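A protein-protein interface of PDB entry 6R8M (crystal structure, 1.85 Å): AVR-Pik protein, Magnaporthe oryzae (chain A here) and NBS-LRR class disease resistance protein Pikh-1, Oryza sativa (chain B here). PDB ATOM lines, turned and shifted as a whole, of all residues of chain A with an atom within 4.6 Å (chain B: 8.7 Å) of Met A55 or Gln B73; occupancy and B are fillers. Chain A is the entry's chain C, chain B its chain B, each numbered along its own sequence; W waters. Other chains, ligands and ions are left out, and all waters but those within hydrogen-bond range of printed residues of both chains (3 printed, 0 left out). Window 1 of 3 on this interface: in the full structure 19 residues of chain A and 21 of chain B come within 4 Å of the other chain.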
ATOM      1  N   TRP A  35     -20.869 -28.881  -2.631  1.00  0.00           N
ATOM      2  CA  TRP A  35     -20.082 -29.515  -3.723  1.00  0.00           C
ATOM      3  C   TRP A  35     -18.769 -28.760  -3.865  1.00  0.00           C
ATOM      4  O   TRP A  35     -18.735 -27.555  -3.606  1.00  0.00           O
ATOM      5  CB  TRP A  35     -20.872 -29.575  -5.023  1.00  0.00           C
ATOM      6  CG  TRP A  35     -21.234 -28.225  -5.589  1.00  0.00           C
ATOM      7  CD1 TRP A  35     -22.456 -27.639  -5.488  1.00  0.00           C
ATOM      8  CD2 TRP A  35     -20.402 -27.301  -6.335  1.00  0.00           C
ATOM      9  NE1 TRP A  35     -22.442 -26.415  -6.103  1.00  0.00           N
ATOM     10  CE2 TRP A  35     -21.192 -26.166  -6.604  1.00  0.00           C
ATOM     11  CE3 TRP A  35     -19.077 -27.326  -6.801  1.00  0.00           C
ATOM     12  CZ2 TRP A  35     -20.720 -25.068  -7.339  1.00  0.00           C
ATOM     13  CZ3 TRP A  35     -18.599 -26.232  -7.496  1.00  0.00           C
ATOM     14  CH2 TRP A  35     -19.410 -25.117  -7.738  1.00  0.00           C
ATOM     15  N   CYS A  49     -25.851 -27.585  -3.449  1.00  0.00           N
ATOM     16  CA  CYS A  49     -26.747 -28.290  -4.349  1.00  0.00           C
ATOM     17  C   CYS A  49     -27.663 -29.173  -3.485  1.00  0.00           C
ATOM     18  O   CYS A  49     -27.330 -29.449  -2.321  1.00  0.00           O
ATOM     19  CB  CYS A  49     -25.989 -29.087  -5.412  1.00  0.00           C
ATOM     20  SG  CYS A  49     -25.017 -30.461  -4.746  1.00  0.00           S
ATOM     21  N   LYS A  54     -30.495 -33.049  -9.224  1.00  0.00           N
ATOM     22  CA  LYS A  54     -29.625 -32.927 -10.414  1.00  0.00           C
ATOM     23  C   LYS A  54     -29.444 -31.447 -10.737  1.00  0.00           C
ATOM     24  O   LYS A  54     -30.289 -30.634 -10.329  1.00  0.00           O
ATOM     25  CB  LYS A  54     -30.230 -33.662 -11.616  1.00  0.00           C
ATOM     26  CG  LYS A  54     -31.591 -33.155 -12.091  1.00  0.00           C
ATOM     27  CD  LYS A  54     -32.777 -33.981 -11.620  1.00  0.00           C
ATOM     28  CE  LYS A  54     -34.098 -33.629 -12.294  1.00  0.00           C
ATOM     29  NZ  LYS A  54     -34.985 -32.865 -11.383  1.00  0.00           N
ATOM     30  N   MET A  55     -28.377 -31.149 -11.448  1.00  0.00           N
ATOM     31  CA  MET A  55     -28.050 -29.780 -11.906  1.00  0.00           C
ATOM     32  C   MET A  55     -27.150 -29.912 -13.141  1.00  0.00           C
ATOM     33  O   MET A  55     -26.436 -30.922 -13.266  1.00  0.00           O
ATOM     34  CB  MET A  55     -27.324 -29.020 -10.792  1.00  0.00           C
ATOM     35  CG  MET A  55     -26.074 -29.678 -10.301  1.00  0.00           C
ATOM     36  SD  MET A  55     -25.200 -28.661  -9.059  1.00  0.00           S
ATOM     37  CE  MET A  55     -24.084 -29.915  -8.413  1.00  0.00           C
ATOM     38  N   ASP A  56     -27.151 -28.896 -13.988  1.00  0.00           N
ATOM     39  CA  ASP A  56     -26.235 -28.831 -15.137  1.00  0.00           C
ATOM     40  C   ASP A  56     -25.183 -27.817 -14.782  1.00  0.00           C
ATOM     41  O   ASP A  56     -25.536 -26.658 -14.433  1.00  0.00           O
ATOM     42  CB  ASP A  56     -26.994 -28.542 -16.422  1.00  0.00           C
ATOM     43  CG  ASP A  56     -27.953 -29.673 -16.764  1.00  0.00           C
ATOM     44  OD1 ASP A  56     -27.591 -30.852 -16.563  1.00  0.00           O
ATOM     45  OD2 ASP A  56     -29.025 -29.364 -17.277  1.00  0.00           O
ATOM     46  N   MET A  57     -23.942 -28.255 -14.856  1.00  0.00           N
ATOM     47  CA  MET A  57     -22.790 -27.435 -14.444  1.00  0.00           C
ATOM     48  C   MET A  57     -21.688 -27.528 -15.490  1.00  0.00           C
ATOM     49  O   MET A  57     -21.408 -28.657 -15.952  1.00  0.00           O
ATOM     50  CB  MET A  57     -22.238 -27.910 -13.108  1.00  0.00           C
ATOM     51  CG  MET A  57     -21.172 -26.975 -12.539  1.00  0.00           C
ATOM     52  SD  MET A  57     -20.560 -27.524 -10.910  1.00  0.00           S
ATOM     53  CE  MET A  57     -22.027 -27.312  -9.924  1.00  0.00           C
ATOM     54  N   TRP A  63     -20.287 -28.899 -20.414  1.00  0.00           N
ATOM     55  CA  TRP A  63     -21.489 -29.011 -19.551  1.00  0.00           C
ATOM     56  C   TRP A  63     -21.626 -30.447 -19.091  1.00  0.00           C
ATOM     57  O   TRP A  63     -21.421 -31.368 -19.905  1.00  0.00           O
ATOM     58  CB  TRP A  63     -22.746 -28.528 -20.262  1.00  0.00           C
ATOM     59  CG  TRP A  63     -22.808 -27.044 -20.322  1.00  0.00           C
ATOM     60  CD1 TRP A  63     -22.439 -26.260 -21.370  1.00  0.00           C
ATOM     61  CD2 TRP A  63     -23.256 -26.157 -19.279  1.00  0.00           C
ATOM     62  NE1 TRP A  63     -22.609 -24.941 -21.055  1.00  0.00           N
ATOM     63  CE2 TRP A  63     -23.154 -24.848 -19.791  1.00  0.00           C
ATOM     64  CE3 TRP A  63     -23.771 -26.340 -17.991  1.00  0.00           C
ATOM     65  CZ2 TRP A  63     -23.514 -23.731 -19.043  1.00  0.00           C
ATOM     66  CZ3 TRP A  63     -24.147 -25.235 -17.257  1.00  0.00           C
ATOM     67  CH2 TRP A  63     -24.003 -23.945 -17.771  1.00  0.00           C
ATOM     68  N   VAL A  64     -21.906 -30.622 -17.815  1.00  0.00           N
ATOM     69  CA  VAL A  64     -22.060 -31.960 -17.199  1.00  0.00           C
ATOM     70  C   VAL A  64     -23.372 -31.988 -16.443  1.00  0.00           C
ATOM     71  O   VAL A  64     -23.603 -31.108 -15.558  1.00  0.00           O
ATOM     72  CB  VAL A  64     -20.886 -32.325 -16.276  1.00  0.00           C
ATOM     73  CG1 VAL A  64     -21.068 -33.722 -15.716  1.00  0.00           C
ATOM     74  CG2 VAL A  64     -19.540 -32.212 -16.940  1.00  0.00           C
ATOM     75  N   HIS A  65     -24.181 -33.004 -16.724  1.00  0.00           N
ATOM     76  CA  HIS A  65     -25.380 -33.321 -15.935  1.00  0.00           C
ATOM     77  C   HIS A  65     -24.941 -34.064 -14.673  1.00  0.00           C
ATOM     78  O   HIS A  65     -24.383 -35.142 -14.808  1.00  0.00           O
ATOM     79  CB  HIS A  65     -26.368 -34.151 -16.783  1.00  0.00           C
ATOM     80  CG  HIS A  65     -27.669 -34.338 -16.105  1.00  0.00           C
ATOM     81  ND1 HIS A  65     -28.541 -33.294 -15.958  1.00  0.00           N
ATOM     82  CD2 HIS A  65     -28.211 -35.399 -15.458  1.00  0.00           C
ATOM     83  CE1 HIS A  65     -29.617 -33.713 -15.313  1.00  0.00           C
ATOM     84  NE2 HIS A  65     -29.441 -35.015 -14.982  1.00  0.00           N
ATOM     85  N   ILE A  66     -25.089 -33.443 -13.497  1.00  0.00           N
ATOM     86  CA  ILE A  66     -24.609 -33.997 -12.213  1.00  0.00           C
ATOM     87  C   ILE A  66     -25.818 -34.414 -11.385  1.00  0.00           C
ATOM     88  O   ILE A  66     -26.706 -33.587 -11.156  1.00  0.00           O
ATOM     89  CB  ILE A  66     -23.744 -32.978 -11.461  1.00  0.00           C
ATOM     90  CG1 ILE A  66     -22.637 -32.459 -12.372  1.00  0.00           C
ATOM     91  CG2 ILE A  66     -23.265 -33.603 -10.154  1.00  0.00           C
ATOM     92  CD1 ILE A  66     -21.678 -31.481 -11.712  1.00  0.00           C
ATOM     93  N   GLN B   6     -35.965 -21.365 -11.047  1.00  0.00           N
ATOM     94  CA  GLN B   6     -34.645 -21.486 -11.671  1.00  0.00           C
ATOM     95  C   GLN B   6     -33.522 -21.033 -10.736  1.00  0.00           C
ATOM     96  O   GLN B   6     -33.693 -20.034  -9.986  1.00  0.00           O
ATOM     97  CB  GLN B   6     -34.609 -20.536 -12.868  1.00  0.00           C
ATOM     98  CG  GLN B   6     -35.616 -20.854 -13.967  1.00  0.00           C
ATOM     99  CD  GLN B   6     -35.596 -19.712 -14.963  1.00  0.00           C
ATOM    100  OE1 GLN B   6     -36.048 -18.597 -14.682  1.00  0.00           O
ATOM    101  NE2 GLN B   6     -34.920 -19.936 -16.077  1.00  0.00           N
ATOM    102  N   LYS B   7     -32.377 -21.684 -10.876  1.00  0.00           N
ATOM    103  CA  LYS B   7     -31.115 -21.229 -10.305  1.00  0.00           C
ATOM    104  C   LYS B   7     -30.139 -21.123 -11.478  1.00  0.00           C
ATOM    105  O   LYS B   7     -29.972 -22.121 -12.254  1.00  0.00           O
ATOM    106  CB  LYS B   7     -30.578 -22.179  -9.251  1.00  0.00           C
ATOM    107  CG  LYS B   7     -29.255 -21.706  -8.657  1.00  0.00           C
ATOM    108  CD  LYS B   7     -28.679 -22.650  -7.660  1.00  0.00           C
ATOM    109  CE  LYS B   7     -29.592 -22.930  -6.487  1.00  0.00           C
ATOM    110  NZ  LYS B   7     -28.941 -23.877  -5.552  1.00  0.00           N
ATOM    111  N   ILE B   8     -29.537 -19.962 -11.615  1.00  0.00           N
ATOM    112  CA  ILE B   8     -28.542 -19.701 -12.682  1.00  0.00           C
ATOM    113  C   ILE B   8     -27.297 -19.138 -12.009  1.00  0.00           C
ATOM    114  O   ILE B   8     -27.467 -18.234 -11.162  1.00  0.00           O
ATOM    115  CB  ILE B   8     -29.146 -18.713 -13.685  1.00  0.00           C
ATOM    116  CG1 ILE B   8     -30.393 -19.285 -14.365  1.00  0.00           C
ATOM    117  CG2 ILE B   8     -28.103 -18.268 -14.686  1.00  0.00           C
ATOM    118  CD1 ILE B   8     -31.259 -18.228 -15.051  1.00  0.00           C
ATOM    119  N   VAL B   9     -26.102 -19.643 -12.354  1.00  0.00           N
ATOM    120  CA  VAL B   9     -24.830 -19.106 -11.809  1.00  0.00           C
ATOM    121  C   VAL B   9     -23.948 -18.621 -12.957  1.00  0.00           C
ATOM    122  O   VAL B   9     -23.810 -19.349 -13.963  1.00  0.00           O
ATOM    123  CB  VAL B   9     -24.080 -20.128 -10.961  1.00  0.00           C
ATOM    124  CG1 VAL B   9     -22.804 -19.538 -10.390  1.00  0.00           C
ATOM    125  CG2 VAL B   9     -24.978 -20.679  -9.869  1.00  0.00           C
ATOM    126  N   ILE B  10     -23.492 -17.389 -12.828  1.00  0.00           N
ATOM    127  CA  ILE B  10     -22.733 -16.653 -13.872  1.00  0.00           C
ATOM    128  C   ILE B  10     -21.406 -16.200 -13.254  1.00  0.00           C
ATOM    129  O   ILE B  10     -21.403 -15.540 -12.210  1.00  0.00           O
ATOM    130  CB  ILE B  10     -23.551 -15.461 -14.443  1.00  0.00           C
ATOM    131  CG1 ILE B  10     -24.847 -15.905 -15.140  1.00  0.00           C
ATOM    132  CG2 ILE B  10     -22.660 -14.671 -15.407  1.00  0.00           C
ATOM    133  CD1 ILE B  10     -25.882 -14.782 -15.355  1.00  0.00           C
ATOM    134  N   LYS B  11     -20.299 -16.462 -13.939  1.00  0.00           N
ATOM    135  CA  LYS B  11     -18.986 -15.911 -13.536  1.00  0.00           C
ATOM    136  C   LYS B  11     -18.805 -14.596 -14.280  1.00  0.00           C
ATOM    137  O   LYS B  11     -19.017 -14.612 -15.486  1.00  0.00           O
ATOM    138  CB  LYS B  11     -17.833 -16.850 -13.870  1.00  0.00           C
ATOM    139  CG  LYS B  11     -16.458 -16.205 -13.699  1.00  0.00           C
ATOM    140  CD  LYS B  11     -15.316 -17.145 -13.981  1.00  0.00           C
ATOM    141  CE  LYS B  11     -15.128 -18.175 -12.884  1.00  0.00           C
ATOM    142  NZ  LYS B  11     -14.680 -17.558 -11.608  1.00  0.00           N
ATOM    143  N   VAL B  39     -21.231 -15.154  -4.779  1.00  0.00           N
ATOM    144  CA  VAL B  39     -20.822 -16.427  -4.155  1.00  0.00           C
ATOM    145  C   VAL B  39     -19.503 -16.858  -4.791  1.00  0.00           C
ATOM    146  O   VAL B  39     -18.975 -16.152  -5.709  1.00  0.00           O
ATOM    147  CB  VAL B  39     -21.928 -17.480  -4.332  1.00  0.00           C
ATOM    148  CG1 VAL B  39     -23.210 -17.041  -3.629  1.00  0.00           C
ATOM    149  CG2 VAL B  39     -22.223 -17.811  -5.776  1.00  0.00           C
ATOM    150  N   LYS B  45     -18.776 -14.932  -8.692  1.00  0.00           N
ATOM    151  CA  LYS B  45     -19.928 -15.625  -9.305  1.00  0.00           C
ATOM    152  C   LYS B  45     -21.191 -14.991  -8.752  1.00  0.00           C
ATOM    153  O   LYS B  45     -21.252 -14.690  -7.538  1.00  0.00           O
ATOM    154  CB  LYS B  45     -19.885 -17.135  -9.009  1.00  0.00           C
ATOM    155  CG  LYS B  45     -18.744 -17.916  -9.656  1.00  0.00           C
ATOM    156  CD  LYS B  45     -18.770 -19.406  -9.345  1.00  0.00           C
ATOM    157  CE  LYS B  45     -18.560 -19.759  -7.877  1.00  0.00           C
ATOM    158  NZ  LYS B  45     -18.823 -21.199  -7.571  1.00  0.00           N
ATOM    159  N   ILE B  46     -22.174 -14.814  -9.625  1.00  0.00           N
ATOM    160  CA  ILE B  46     -23.516 -14.338  -9.240  1.00  0.00           C
ATOM    161  C   ILE B  46     -24.458 -15.547  -9.341  1.00  0.00           C
ATOM    162  O   ILE B  46     -24.604 -16.147 -10.432  1.00  0.00           O
ATOM    163  CB  ILE B  46     -23.969 -13.134 -10.080  1.00  0.00           C
ATOM    164  CG1 ILE B  46     -22.976 -11.975  -9.965  1.00  0.00           C
ATOM    165  CG2 ILE B  46     -25.380 -12.722  -9.681  1.00  0.00           C
ATOM    166  CD1 ILE B  46     -23.355 -10.747 -10.784  1.00  0.00           C
ATOM    167  N   GLU B  47     -25.075 -15.875  -8.221  1.00  0.00           N
ATOM    168  CA  GLU B  47     -26.164 -16.886  -8.178  1.00  0.00           C
ATOM    169  C   GLU B  47     -27.476 -16.124  -8.234  1.00  0.00           C
ATOM    170  O   GLU B  47     -27.707 -15.234  -7.407  1.00  0.00           O
ATOM    171  CB  GLU B  47     -26.033 -17.812  -6.959  1.00  0.00           C
ATOM    172  CG  GLU B  47     -27.141 -18.818  -6.889  1.00  0.00           C
ATOM    173  CD  GLU B  47     -27.065 -19.828  -5.746  1.00  0.00           C
ATOM    174  OE1 GLU B  47     -28.134 -20.127  -5.179  1.00  0.00           O
ATOM    175  OE2 GLU B  47     -25.970 -20.323  -5.449  1.00  0.00           O
ATOM    176  N   VAL B  48     -28.276 -16.435  -9.234  1.00  0.00           N
ATOM    177  CA  VAL B  48     -29.606 -15.792  -9.410  1.00  0.00           C
ATOM    178  C   VAL B  48     -30.685 -16.865  -9.267  1.00  0.00           C
ATOM    179  O   VAL B  48     -30.553 -17.994  -9.826  1.00  0.00           O
ATOM    180  CB  VAL B  48     -29.768 -14.968 -10.708  1.00  0.00           C
ATOM    181  CG1 VAL B  48     -29.609 -15.795 -11.958  1.00  0.00           C
ATOM    182  CG2 VAL B  48     -31.106 -14.248 -10.742  1.00  0.00           C
ATOM    183  N   PRO B  55     -31.411 -17.384 -19.633  1.00  0.00           N
ATOM    184  CA  PRO B  55     -30.022 -17.267 -19.222  1.00  0.00           C
ATOM    185  C   PRO B  55     -29.113 -16.789 -20.365  1.00  0.00           C
ATOM    186  O   PRO B  55     -28.153 -16.158 -20.078  1.00  0.00           O
ATOM    187  CB  PRO B  55     -29.584 -18.655 -18.775  1.00  0.00           C
ATOM    188  CG  PRO B  55     -30.732 -19.578 -19.119  1.00  0.00           C
ATOM    189  CD  PRO B  55     -31.922 -18.752 -19.567  1.00  0.00           C
ATOM    190  N   ILE B  59     -26.747 -13.418 -20.258  1.00  0.00           N
ATOM    191  CA  ILE B  59     -25.287 -13.460 -20.544  1.00  0.00           C
ATOM    192  C   ILE B  59     -24.962 -12.393 -21.607  1.00  0.00           C
ATOM    193  O   ILE B  59     -23.970 -11.653 -21.401  1.00  0.00           O
ATOM    194  CB  ILE B  59     -24.849 -14.878 -20.976  1.00  0.00           C
ATOM    195  CG1 ILE B  59     -24.735 -15.820 -19.780  1.00  0.00           C
ATOM    196  CG2 ILE B  59     -23.547 -14.853 -21.769  1.00  0.00           C
ATOM    197  CD1 ILE B  59     -23.493 -15.582 -18.937  1.00  0.00           C
ATOM    198  N   GLU B  70     -19.528 -15.764 -18.085  1.00  0.00           N
ATOM    199  CA  GLU B  70     -19.618 -17.168 -18.520  1.00  0.00           C
ATOM    200  C   GLU B  70     -20.747 -17.823 -17.708  1.00  0.00           C
ATOM    201  O   GLU B  70     -20.796 -17.608 -16.490  1.00  0.00           O
ATOM    202  CB  GLU B  70     -18.242 -17.790 -18.325  1.00  0.00           C
ATOM    203  CG  GLU B  70     -18.135 -19.236 -18.789  1.00  0.00           C
ATOM    204  CD  GLU B  70     -16.957 -20.022 -18.227  1.00  0.00           C
ATOM    205  OE1 GLU B  70     -16.136 -19.414 -17.480  1.00  0.00           O
ATOM    206  OE2 GLU B  70     -16.878 -21.257 -18.494  1.00  0.00           O
ATOM    207  N   LEU B  71     -21.648 -18.537 -18.376  1.00  0.00           N
ATOM    208  CA  LEU B  71     -22.739 -19.272 -17.707  1.00  0.00           C
ATOM    209  C   LEU B  71     -22.110 -20.526 -17.103  1.00  0.00           C
ATOM    210  O   LEU B  71     -21.406 -21.243 -17.826  1.00  0.00           O
ATOM    211  CB  LEU B  71     -23.804 -19.587 -18.756  1.00  0.00           C
ATOM    212  CG  LEU B  71     -25.076 -20.246 -18.242  1.00  0.00           C
ATOM    213  CD1 LEU B  71     -25.731 -19.383 -17.166  1.00  0.00           C
ATOM    214  CD2 LEU B  71     -26.050 -20.515 -19.391  1.00  0.00           C
ATOM    215  N   LEU B  72     -22.320 -20.785 -15.816  1.00  0.00           N
ATOM    216  CA  LEU B  72     -21.654 -21.917 -15.115  1.00  0.00           C
ATOM    217  C   LEU B  72     -22.655 -22.976 -14.648  1.00  0.00           C
ATOM    218  O   LEU B  72     -22.221 -24.119 -14.426  1.00  0.00           O
ATOM    219  CB  LEU B  72     -20.899 -21.381 -13.903  1.00  0.00           C
ATOM    220  CG  LEU B  72     -19.680 -20.505 -14.169  1.00  0.00           C
ATOM    221  CD1 LEU B  72     -18.899 -20.297 -12.856  1.00  0.00           C
ATOM    222  CD2 LEU B  72     -18.795 -21.104 -15.251  1.00  0.00           C
ATOM    223  N   GLN B  73     -23.927 -22.606 -14.433  1.00  0.00           N
ATOM    224  CA  GLN B  73     -24.904 -23.557 -13.849  1.00  0.00           C
ATOM    225  C   GLN B  73     -26.304 -23.117 -14.238  1.00  0.00           C
ATOM    226  O   GLN B  73     -26.591 -21.895 -14.257  1.00  0.00           O
ATOM    227  CB  GLN B  73     -24.808 -23.610 -12.325  1.00  0.00           C
ATOM    228  CG  GLN B  73     -25.597 -24.757 -11.682  1.00  0.00           C
ATOM    229  CD  GLN B  73     -25.475 -24.715 -10.168  1.00  0.00           C
ATOM    230  OE1 GLN B  73     -24.393 -24.426  -9.601  1.00  0.00           O
ATOM    231  NE2 GLN B  73     -26.580 -25.085  -9.516  1.00  0.00           N
ATOM    232  N   VAL B  74     -27.128 -24.085 -14.595  1.00  0.00           N
ATOM    233  CA  VAL B  74     -28.594 -23.887 -14.731  1.00  0.00           C
ATOM    234  C   VAL B  74     -29.239 -25.094 -14.081  1.00  0.00           C
ATOM    235  O   VAL B  74     -28.847 -26.256 -14.391  1.00  0.00           O
ATOM    236  CB  VAL B  74     -29.054 -23.719 -16.182  1.00  0.00           C
ATOM    237  CG1 VAL B  74     -30.572 -23.579 -16.249  1.00  0.00           C
ATOM    238  CG2 VAL B  74     -28.342 -22.556 -16.865  1.00  0.00           C
ATOM    239  N   SER B  75     -30.086 -24.827 -13.093  1.00  0.00           N
ATOM    240  CA  SER B  75     -30.720 -25.899 -12.327  1.00  0.00           C
ATOM    241  C   SER B  75     -32.094 -25.416 -11.885  1.00  0.00           C
ATOM    242  O   SER B  75     -32.470 -24.234 -12.177  1.00  0.00           O
ATOM    243  CB  SER B  75     -29.825 -26.365 -11.194  1.00  0.00           C
ATOM    244  OG  SER B  75     -29.463 -25.320 -10.302  1.00  0.00           O
ATOM    245  N   GLN B  76     -32.826 -26.301 -11.238  1.00  0.00           N
ATOM    246  CA  GLN B  76     -34.165 -25.988 -10.703  1.00  0.00           C
ATOM    247  C   GLN B  76     -34.101 -26.155  -9.197  1.00  0.00           C
ATOM    248  O   GLN B  76     -33.291 -26.966  -8.683  1.00  0.00           O
ATOM    249  CB  GLN B  76     -35.227 -26.906 -11.298  1.00  0.00           C
ATOM    250  CG  GLN B  76     -35.301 -26.910 -12.801  1.00  0.00           C
ATOM    251  CD  GLN B  76     -36.468 -27.789 -13.161  1.00  0.00           C
ATOM    252  OE1 GLN B  76     -36.400 -29.014 -13.016  1.00  0.00           O
ATOM    253  NE2 GLN B  76     -37.554 -27.158 -13.582  1.00  0.00           N
ATOM    254  N   ALA B  77     -34.929 -25.409  -8.495  1.00  0.00           N
ATOM    255  CA  ALA B  77     -35.067 -25.551  -7.037  1.00  0.00           C
ATOM    256  C   ALA B  77     -35.907 -26.812  -6.776  1.00  0.00           C
ATOM    257  O   ALA B  77     -36.946 -26.980  -7.436  1.00  0.00           O
ATOM    258  CB  ALA B  77     -35.705 -24.328  -6.446  1.00  0.00           C
HETATM  259  O   HOH W   1     -24.074 -24.078  -6.849  1.00  0.00           O
HETATM  260  O   HOH W   2     -30.503 -27.564 -16.125  1.00  0.00           O
HETATM  261  O   HOH W   3     -32.168 -29.140 -11.493  1.00  0.00           O
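The backbone carbonyl oxygen (O) of Asp A56 sits at hydrogen-bond distance from the backbone NH (N) of Val B74.
The backbone NH of Ile A66 is in hydrogen-bond range of the backbone carbonyl oxygen of Met A55, at 2.9 Å.
The side-chain carboxylate of Asp A56 lies within hydrogen-bond range of a ring nitrogen (ND1) of His A65 (2.7 Å).
The backbone carbonyl oxygen of Lys B45 is in hydrogen-bond range of the backbone NH of Val B39 (2.8 Å).
The backbone carbonyl oxygen (O) of Met A57 sits at hydrogen-bond distance from the backbone NH (N) of Val A64 (2.8 Å).
OG of Ser B75 is in hydrogen-bond range of NE2 of Gln B73 (3.0 Å).
O of Gln B73 sits at hydrogen-bond distance from N of Val B9 (3.0 Å).
Among the printed residues, pairs that only touch across the chains: Trp A35 with Lys B45, Met A55 with Gln B73, Met A55 with Ser B75, Asp A56 with Gln B73, Met A57 with Leu B72, Met A57 with Gln B73, Trp A63 with Leu B71, Trp A63 with Leu B72 and Trp A63 with Gln B73.
Met A55 touches just these residues of chain B: Gln B73 and Ser B75.
Gln B73 touches just these residues of chain A: Met A55 (3.9 Å), Asp A56 (3.2 Å), Met A57 (3.7 Å) and Trp A63 (3.6 Å).
Asp A56 touches just these residues of chain B: Gln B73 and Val B74.
No residue of chain B comes within 4 Å of Ile A66.
Of the printed residues of chain A, Val B74 touches Asp A56 (3.0 Å).
Of the printed residues of chain A, Ser B75 touches Met A55 (3.7 Å).
Of the printed residues of chain A, Lys B45 touches Trp A35 (3.97 Å).
Of the printed residues of chain B, Trp A63 touches Leu B71 (3.5 Å), Leu B72 (3.5 Å) and Gln B73 (3.6 Å).
Glu B47 touches none of the printed residues of chain A.
The nearest residue of chain B that does not touch Met A55 is Val B74 (4.2 Å).
The nearest residue of chain A that does not touch Gln B73 is Trp A35 (4.4 Å).
Of the 10 printed residues of chain A, 5 touch a printed residue of chain B.
Printed residues of chain A that touch a printed residue of chain B: Trp A35, Met A55, Asp A56, Met A57 and Trp A63.
Of the 21 printed residues of chain B, 6 touch a printed residue of chain A.
Printed residues of chain B that touch a printed residue of chain A: Lys B45, Leu B71, Leu B72, Gln B73, Val B74 and Ser B75.
Hydrophobic or aromatic side chains of chain B within 4 Å of the printed part of chain A: Leu B71.
Among the printed residues, 10 pairs touch across the chains.
Among the printed residues, no Asp or Glu carboxylate lies within 4 Å of a Lys or Arg side-chain nitrogen of the other chain.
Water W2 bridges OD2 of Asp A56 (2.6 Å) and O of Val B74 (2.7 Å).
Water W3 bridges O of Lys A54 (2.7 Å) and N of Gln B76 (2.9 Å).
Water W1 bridges OE1 of Gln B73 and NE1 of Trp A35.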
